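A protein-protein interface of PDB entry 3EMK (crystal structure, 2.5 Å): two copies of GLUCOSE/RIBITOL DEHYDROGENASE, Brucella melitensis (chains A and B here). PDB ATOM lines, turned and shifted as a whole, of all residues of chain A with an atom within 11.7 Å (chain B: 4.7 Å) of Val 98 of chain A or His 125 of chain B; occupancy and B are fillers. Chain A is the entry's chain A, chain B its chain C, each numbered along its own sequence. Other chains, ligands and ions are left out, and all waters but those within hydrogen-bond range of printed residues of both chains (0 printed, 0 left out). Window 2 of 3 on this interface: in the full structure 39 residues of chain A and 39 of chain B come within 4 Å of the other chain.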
ATOM      1  N   ARG A  93     -14.264   0.053  28.065  1.00  0.00           N
ATOM      2  CA  ARG A  93     -13.017   0.231  27.333  1.00  0.00           C
ATOM      3  C   ARG A  93     -12.103   0.985  28.269  1.00  0.00           C
ATOM      4  O   ARG A  93     -11.909   2.169  28.072  1.00  0.00           O
ATOM      5  CB  ARG A  93     -13.210   1.088  26.061  1.00  0.00           C
ATOM      6  CG  ARG A  93     -14.022   0.467  24.928  1.00  0.00           C
ATOM      7  CD  ARG A  93     -13.337  -0.725  24.279  1.00  0.00           C
ATOM      8  NE  ARG A  93     -14.297  -1.832  24.189  1.00  0.00           N
ATOM      9  CZ  ARG A  93     -14.929  -2.220  23.083  1.00  0.00           C
ATOM     10  NH1 ARG A  93     -14.705  -1.613  21.920  1.00  0.00           N
ATOM     11  NH2 ARG A  93     -15.776  -3.238  23.152  1.00  0.00           N
ATOM     12  N   ASP A  94     -11.561   0.317  29.287  1.00  0.00           N
ATOM     13  CA  ASP A  94     -10.826   1.015  30.348  1.00  0.00           C
ATOM     14  C   ASP A  94      -9.445   1.397  29.865  1.00  0.00           C
ATOM     15  O   ASP A  94      -8.858   0.712  29.016  1.00  0.00           O
ATOM     16  CB  ASP A  94     -10.668   0.162  31.621  1.00  0.00           C
ATOM     17  CG  ASP A  94     -11.989  -0.109  32.360  1.00  0.00           C
ATOM     18  OD1 ASP A  94     -13.077   0.448  32.024  1.00  0.00           O
ATOM     19  OD2 ASP A  94     -11.927  -0.908  33.327  1.00  0.00           O
ATOM     20  N   GLY A  95      -8.915   2.472  30.443  1.00  0.00           N
ATOM     21  CA  GLY A  95      -7.562   2.972  30.132  1.00  0.00           C
ATOM     22  C   GLY A  95      -7.433   4.388  30.664  1.00  0.00           C
ATOM     23  O   GLY A  95      -8.435   5.009  31.004  1.00  0.00           O
ATOM     24  N   LEU A  96      -6.206   4.893  30.763  1.00  0.00           N
ATOM     25  CA  LEU A  96      -5.992   6.255  31.234  1.00  0.00           C
ATOM     26  C   LEU A  96      -6.549   7.217  30.183  1.00  0.00           C
ATOM     27  O   LEU A  96      -6.597   6.889  28.985  1.00  0.00           O
ATOM     28  CB  LEU A  96      -4.503   6.523  31.572  1.00  0.00           C
ATOM     29  CG  LEU A  96      -3.925   5.882  32.862  1.00  0.00           C
ATOM     30  CD1 LEU A  96      -2.422   6.118  33.031  1.00  0.00           C
ATOM     31  CD2 LEU A  96      -4.659   6.339  34.134  1.00  0.00           C
ATOM     32  N   PHE A  97      -7.009   8.381  30.644  1.00  0.00           N
ATOM     33  CA  PHE A  97      -7.649   9.368  29.764  1.00  0.00           C
ATOM     34  C   PHE A  97      -6.691   9.868  28.686  1.00  0.00           C
ATOM     35  O   PHE A  97      -7.074  10.051  27.521  1.00  0.00           O
ATOM     36  CB  PHE A  97      -8.202  10.556  30.573  1.00  0.00           C
ATOM     37  CG  PHE A  97      -8.686  11.715  29.722  1.00  0.00           C
ATOM     38  CD1 PHE A  97      -9.877  11.622  28.998  1.00  0.00           C
ATOM     39  CD2 PHE A  97      -7.951  12.896  29.649  1.00  0.00           C
ATOM     40  CE1 PHE A  97     -10.314  12.679  28.219  1.00  0.00           C
ATOM     41  CE2 PHE A  97      -8.387  13.966  28.881  1.00  0.00           C
ATOM     42  CZ  PHE A  97      -9.568  13.862  28.166  1.00  0.00           C
ATOM     43  N   VAL A  98      -5.445  10.078  29.088  1.00  0.00           N
ATOM     44  CA  VAL A  98      -4.480  10.726  28.211  1.00  0.00           C
ATOM     45  C   VAL A  98      -3.994   9.769  27.123  1.00  0.00           C
ATOM     46  O   VAL A  98      -3.360  10.181  26.171  1.00  0.00           O
ATOM     47  CB  VAL A  98      -3.305  11.328  28.995  1.00  0.00           C
ATOM     48  CG1 VAL A  98      -2.778  12.516  28.243  1.00  0.00           C
ATOM     49  CG2 VAL A  98      -3.762  11.778  30.351  1.00  0.00           C
ATOM     50  N   ARG A  99      -4.336   8.493  27.272  1.00  0.00           N
ATOM     51  CA  ARG A  99      -4.059   7.473  26.269  1.00  0.00           C
ATOM     52  C   ARG A  99      -5.348   7.005  25.581  1.00  0.00           C
ATOM     53  O   ARG A  99      -5.304   6.092  24.752  1.00  0.00           O
ATOM     54  CB  ARG A  99      -3.333   6.276  26.919  1.00  0.00           C
ATOM     55  CG  ARG A  99      -1.891   6.546  27.448  1.00  0.00           C
ATOM     56  CD  ARG A  99      -1.460   5.378  28.392  1.00  0.00           C
ATOM     57  NE  ARG A  99      -0.076   5.455  28.907  1.00  0.00           N
ATOM     58  CZ  ARG A  99       0.330   4.949  30.086  1.00  0.00           C
ATOM     59  NH1 ARG A  99      -0.543   4.342  30.900  1.00  0.00           N
ATOM     60  NH2 ARG A  99       1.613   5.058  30.469  1.00  0.00           N
ATOM     61  N   MET A 100      -6.483   7.619  25.916  1.00  0.00           N
ATOM     62  CA  MET A 100      -7.792   7.099  25.492  1.00  0.00           C
ATOM     63  C   MET A 100      -8.110   7.507  24.057  1.00  0.00           C
ATOM     64  O   MET A 100      -8.042   8.682  23.714  1.00  0.00           O
ATOM     65  CB  MET A 100      -8.909   7.531  26.457  1.00  0.00           C
ATOM     66  CG  MET A 100     -10.287   6.946  26.158  1.00  0.00           C
ATOM     67  SD  MET A 100     -11.599   7.418  27.337  1.00  0.00           S
ATOM     68  CE  MET A 100     -11.069   6.586  28.821  1.00  0.00           C
ATOM     69  N   SER A 101      -8.459   6.536  23.222  1.00  0.00           N
ATOM     70  CA  SER A 101      -8.669   6.798  21.795  1.00  0.00           C
ATOM     71  C   SER A 101     -10.125   7.162  21.518  1.00  0.00           C
ATOM     72  O   SER A 101     -11.022   6.816  22.310  1.00  0.00           O
ATOM     73  CB  SER A 101      -8.266   5.590  20.962  1.00  0.00           C
ATOM     74  OG  SER A 101      -9.277   4.607  21.011  1.00  0.00           O
ATOM     75  N   ASP A 102     -10.362   7.856  20.410  1.00  0.00           N
ATOM     76  CA  ASP A 102     -11.725   8.208  20.012  1.00  0.00           C
ATOM     77  C   ASP A 102     -12.619   6.984  19.988  1.00  0.00           C
ATOM     78  O   ASP A 102     -13.767   7.035  20.426  1.00  0.00           O
ATOM     79  CB  ASP A 102     -11.753   8.870  18.631  1.00  0.00           C
ATOM     80  CG  ASP A 102     -10.929  10.144  18.564  1.00  0.00           C
ATOM     81  OD1 ASP A 102     -10.713  10.836  19.592  1.00  0.00           O
ATOM     82  OD2 ASP A 102     -10.497  10.474  17.448  1.00  0.00           O
ATOM     83  N   ASP A 104     -12.434   4.237  21.634  1.00  0.00           N
ATOM     84  CA  ASP A 104     -12.740   3.790  22.996  1.00  0.00           C
ATOM     85  C   ASP A 104     -13.782   4.653  23.717  1.00  0.00           C
ATOM     86  O   ASP A 104     -14.518   4.164  24.571  1.00  0.00           O
ATOM     87  CB  ASP A 104     -11.457   3.701  23.836  1.00  0.00           C
ATOM     88  CG  ASP A 104     -10.643   2.466  23.528  1.00  0.00           C
ATOM     89  OD1 ASP A 104     -11.159   1.527  22.875  1.00  0.00           O
ATOM     90  OD2 ASP A 104      -9.477   2.435  23.960  1.00  0.00           O
ATOM     91  N   TRP A 105     -13.830   5.934  23.376  1.00  0.00           N
ATOM     92  CA  TRP A 105     -14.813   6.842  23.934  1.00  0.00           C
ATOM     93  C   TRP A 105     -16.123   6.574  23.198  1.00  0.00           C
ATOM     94  O   TRP A 105     -17.135   6.195  23.830  1.00  0.00           O
ATOM     95  CB  TRP A 105     -14.334   8.298  23.795  1.00  0.00           C
ATOM     96  CG  TRP A 105     -15.371   9.301  24.108  1.00  0.00           C
ATOM     97  CD1 TRP A 105     -16.258   9.850  23.229  1.00  0.00           C
ATOM     98  CD2 TRP A 105     -15.668   9.875  25.391  1.00  0.00           C
ATOM     99  NE1 TRP A 105     -17.084  10.729  23.879  1.00  0.00           N
ATOM    100  CE2 TRP A 105     -16.752  10.763  25.208  1.00  0.00           C
ATOM    101  CE3 TRP A 105     -15.124   9.729  26.679  1.00  0.00           C
ATOM    102  CZ2 TRP A 105     -17.307  11.510  26.267  1.00  0.00           C
ATOM    103  CZ3 TRP A 105     -15.675  10.471  27.733  1.00  0.00           C
ATOM    104  CH2 TRP A 105     -16.756  11.344  27.518  1.00  0.00           C
ATOM    105  N   ASN A 147     -14.171   7.310  38.818  1.00  0.00           N
ATOM    106  CA  ASN A 147     -13.148   6.275  38.999  1.00  0.00           C
ATOM    107  C   ASN A 147     -12.053   6.490  37.955  1.00  0.00           C
ATOM    108  O   ASN A 147     -12.359   6.681  36.786  1.00  0.00           O
ATOM    109  CB  ASN A 147     -13.781   4.900  38.819  1.00  0.00           C
ATOM    110  CG  ASN A 147     -12.914   3.745  39.316  1.00  0.00           C
ATOM    111  OD1 ASN A 147     -12.117   3.878  40.245  1.00  0.00           O
ATOM    112  ND2 ASN A 147     -13.107   2.587  38.713  1.00  0.00           N
ATOM    113  N   PRO A 148     -10.769   6.461  38.367  1.00  0.00           N
ATOM    114  CA  PRO A 148      -9.678   6.527  37.403  1.00  0.00           C
ATOM    115  C   PRO A 148      -9.757   5.351  36.431  1.00  0.00           C
ATOM    116  O   PRO A 148     -10.250   4.290  36.798  1.00  0.00           O
ATOM    117  CB  PRO A 148      -8.439   6.391  38.281  1.00  0.00           C
ATOM    118  CG  PRO A 148      -8.915   5.707  39.528  1.00  0.00           C
ATOM    119  CD  PRO A 148     -10.262   6.314  39.743  1.00  0.00           C
ATOM    120  N   GLY A 149      -9.310   5.547  35.195  1.00  0.00           N
ATOM    121  CA  GLY A 149      -9.323   4.487  34.191  1.00  0.00           C
ATOM    122  C   GLY A 149     -10.620   4.410  33.396  1.00  0.00           C
ATOM    123  O   GLY A 149     -10.712   3.665  32.439  1.00  0.00           O
ATOM    124  N   GLN A 150     -11.627   5.191  33.764  1.00  0.00           N
ATOM    125  CA  GLN A 150     -12.955   4.990  33.188  1.00  0.00           C
ATOM    126  C   GLN A 150     -13.664   6.291  32.891  1.00  0.00           C
ATOM    127  O   GLN A 150     -14.871   6.395  33.119  1.00  0.00           O
ATOM    128  CB  GLN A 150     -13.832   4.164  34.145  1.00  0.00           C
ATOM    129  CG  GLN A 150     -13.266   2.809  34.584  1.00  0.00           C
ATOM    130  CD  GLN A 150     -14.334   1.931  35.210  1.00  0.00           C
ATOM    131  OE1 GLN A 150     -14.658   2.051  36.407  1.00  0.00           O
ATOM    132  NE2 GLN A 150     -14.906   1.058  34.402  1.00  0.00           N
ATOM    133  N   ALA A 151     -12.924   7.280  32.385  1.00  0.00           N
ATOM    134  CA  ALA A 151     -13.500   8.577  32.044  1.00  0.00           C
ATOM    135  C   ALA A 151     -14.737   8.391  31.172  1.00  0.00           C
ATOM    136  O   ALA A 151     -15.807   8.927  31.480  1.00  0.00           O
ATOM    137  CB  ALA A 151     -12.472   9.456  31.353  1.00  0.00           C
ATOM    138  N   ASN A 152     -14.584   7.603  30.107  1.00  0.00           N
ATOM    139  CA  ASN A 152     -15.693   7.239  29.218  1.00  0.00           C
ATOM    140  C   ASN A 152     -16.854   6.503  29.897  1.00  0.00           C
ATOM    141  O   ASN A 152     -18.006   6.866  29.694  1.00  0.00           O
ATOM    142  CB  ASN A 152     -15.190   6.436  27.997  1.00  0.00           C
ATOM    143  CG  ASN A 152     -14.409   5.146  28.376  1.00  0.00           C
ATOM    144  OD1 ASN A 152     -14.176   4.842  29.549  1.00  0.00           O
ATOM    145  ND2 ASN A 152     -13.992   4.402  27.353  1.00  0.00           N
ATOM    146  N   LEU B 123      -5.239  18.899  25.680  1.00  0.00           N
ATOM    147  CA  LEU B 123      -4.505  19.820  26.568  1.00  0.00           C
ATOM    148  C   LEU B 123      -4.076  19.295  27.935  1.00  0.00           C
ATOM    149  O   LEU B 123      -3.230  19.920  28.579  1.00  0.00           O
ATOM    150  CB  LEU B 123      -5.293  21.122  26.779  1.00  0.00           C
ATOM    151  CG  LEU B 123      -5.749  21.914  25.551  1.00  0.00           C
ATOM    152  CD1 LEU B 123      -6.652  23.043  25.969  1.00  0.00           C
ATOM    153  CD2 LEU B 123      -4.578  22.423  24.727  1.00  0.00           C
ATOM    154  N   THR B 124      -4.653  18.190  28.402  1.00  0.00           N
ATOM    155  CA  THR B 124      -4.377  17.759  29.783  1.00  0.00           C
ATOM    156  C   THR B 124      -2.936  17.275  29.960  1.00  0.00           C
ATOM    157  O   THR B 124      -2.241  17.715  30.867  1.00  0.00           O
ATOM    158  CB  THR B 124      -5.430  16.748  30.391  1.00  0.00           C
ATOM    159  OG1 THR B 124      -5.229  15.435  29.873  1.00  0.00           O
ATOM    160  CG2 THR B 124      -6.832  17.171  30.094  1.00  0.00           C
ATOM    161  N   HIS B 125      -2.464  16.405  29.081  1.00  0.00           N
ATOM    162  CA  HIS B 125      -1.071  15.943  29.181  1.00  0.00           C
ATOM    163  C   HIS B 125      -0.052  17.097  29.274  1.00  0.00           C
ATOM    164  O   HIS B 125       0.748  17.138  30.212  1.00  0.00           O
ATOM    165  CB  HIS B 125      -0.704  14.950  28.075  1.00  0.00           C
ATOM    166  CG  HIS B 125       0.515  14.150  28.384  1.00  0.00           C
ATOM    167  ND1 HIS B 125       0.559  13.245  29.420  1.00  0.00           N
ATOM    168  CD2 HIS B 125       1.749  14.151  27.829  1.00  0.00           C
ATOM    169  CE1 HIS B 125       1.760  12.699  29.475  1.00  0.00           C
ATOM    170  NE2 HIS B 125       2.505  13.239  28.526  1.00  0.00           N
ATOM    171  N   PRO B 126      -0.096  18.052  28.324  1.00  0.00           N
ATOM    172  CA  PRO B 126       0.705  19.263  28.479  1.00  0.00           C
ATOM    173  C   PRO B 126       0.577  19.912  29.861  1.00  0.00           C
ATOM    174  O   PRO B 126       1.597  20.168  30.509  1.00  0.00           O
ATOM    175  CB  PRO B 126       0.149  20.169  27.386  1.00  0.00           C
ATOM    176  CG  PRO B 126      -0.175  19.205  26.296  1.00  0.00           C
ATOM    177  CD  PRO B 126      -0.836  18.071  27.046  1.00  0.00           C
ATOM    178  N   MET B 127      -0.654  20.147  30.318  1.00  0.00           N
ATOM    179  CA  MET B 127      -0.863  20.651  31.678  1.00  0.00           C
ATOM    180  C   MET B 127      -0.173  19.809  32.753  1.00  0.00           C
ATOM    181  O   MET B 127       0.468  20.366  33.619  1.00  0.00           O
ATOM    182  CB  MET B 127      -2.337  20.776  32.002  1.00  0.00           C
ATOM    183  CG  MET B 127      -3.002  21.976  31.422  1.00  0.00           C
ATOM    184  SD  MET B 127      -4.740  21.874  31.830  1.00  0.00           S
ATOM    185  CE  MET B 127      -5.445  23.164  30.814  1.00  0.00           C
ATOM    186  N   MET B 128      -0.305  18.484  32.690  1.00  0.00           N
ATOM    187  CA  MET B 128       0.300  17.581  33.678  1.00  0.00           C
ATOM    188  C   MET B 128       1.823  17.675  33.653  1.00  0.00           C
ATOM    189  O   MET B 128       2.457  17.722  34.703  1.00  0.00           O
ATOM    190  CB  MET B 128      -0.136  16.132  33.438  1.00  0.00           C
ATOM    191  CG  MET B 128      -1.642  15.925  33.361  1.00  0.00           C
ATOM    192  SD  MET B 128      -2.179  14.248  32.984  1.00  0.00           S
ATOM    193  CE  MET B 128      -1.049  13.771  31.701  1.00  0.00           C
ATOM    194  N   ARG B 129       2.395  17.702  32.443  1.00  0.00           N
ATOM    195  CA  ARG B 129       3.831  17.893  32.242  1.00  0.00           C
ATOM    196  C   ARG B 129       4.311  19.199  32.884  1.00  0.00           C
ATOM    197  O   ARG B 129       5.394  19.236  33.478  1.00  0.00           O
ATOM    198  CB  ARG B 129       4.171  17.888  30.746  1.00  0.00           C
ATOM    199  CG  ARG B 129       4.094  16.511  30.043  1.00  0.00           C
ATOM    200  CD  ARG B 129       5.476  16.012  29.662  1.00  0.00           C
ATOM    201  NE  ARG B 129       5.886  16.459  28.331  1.00  0.00           N
ATOM    202  CZ  ARG B 129       7.144  16.720  27.957  1.00  0.00           C
ATOM    203  NH1 ARG B 129       8.165  16.624  28.815  1.00  0.00           N
ATOM    204  NH2 ARG B 129       7.382  17.105  26.713  1.00  0.00           N
ATOM    205  N   GLU B 170      -7.797  10.692  38.170  1.00  0.00           N
ATOM    206  CA  GLU B 170      -6.601  10.271  37.466  1.00  0.00           C
ATOM    207  C   GLU B 170      -5.435  11.225  37.665  1.00  0.00           C
ATOM    208  O   GLU B 170      -4.308  10.789  37.831  1.00  0.00           O
ATOM    209  CB  GLU B 170      -6.875  10.109  35.970  1.00  0.00           C
ATOM    210  CG  GLU B 170      -7.773   8.941  35.606  1.00  0.00           C
ATOM    211  CD  GLU B 170      -7.796   8.678  34.122  1.00  0.00           C
ATOM    212  OE1 GLU B 170      -8.655   7.874  33.663  1.00  0.00           O
ATOM    213  OE2 GLU B 170      -6.952   9.275  33.413  1.00  0.00           O
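Of chain B, only Thr 124, His 125 and Met 128 come within 4 Å of Val 98 of chain A. Of chain A, only Val 98 comes within 4 Å of His 125 of chain B. Of the printed residues of chain A, Thr 124 of chain B touches Phe 97 (3.6 Å) and Val 98 (3.97 Å). No residue of chain A comes within 4 Å of Pro 126 of chain B. Of the printed residues of chain A, Met 128 of chain B touches Val 98. Printed residues of chain B within 4 Å of Pro 148 of chain A: Glu 170. Of the printed residues of chain B, Gly 95 of chain A touches Glu 170. Of the printed residues of chain B, Gly 149 of chain A touches Glu 170 (2.9 Å). Asp 104 of chain A touches none of the printed residues of chain B. Asp 102 of chain A touches none of the printed residues of chain B. The nearest residue of chain A that does not touch His 125 of chain B is Phe 97 of chain A (6.4 Å).
Hydrophobic or aromatic side chains of chain A within 4 Å of the printed part of chain B: Leu 96, Phe 97, Val 98 and Pro 148. Of the 8 printed residues of chain B, 4 touch a printed residue of chain A. Hydrophobic or aromatic side chains of chain B that line the printed part of chain A: His 125 and Met 128.
Among the printed residues, pairs that only touch across the chains: Val 98 of chain A with His 125 of chain B (3.2 Å), Pro 148 of chain A with Glu 170 of chain B (3.6 Å), Phe 97 of chain A with Thr 124 of chain B (3.6 Å), Val 98 of chain A with Met 128 of chain B (3.6 Å), Leu 96 of chain A with Glu 170 of chain B (3.8 Å), Gly 95 of chain A with Glu 170 of chain B (3.9 Å) and Val 98 of chain A with Thr 124 of chain B (3.97 Å).
N of Gly 149 of chain A is in hydrogen-bond range of OE1 of Glu 170 of chain B. N of Phe 97 of chain A lies within hydrogen-bond range of OE2 of Glu 170 of chain B (2.9 Å).
No position is printed for both chains.
The backbone NH (N) of Gly 95 of chain A lies within hydrogen-bond range of the backbone carbonyl oxygen (O) of Gly 149 of chain A.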
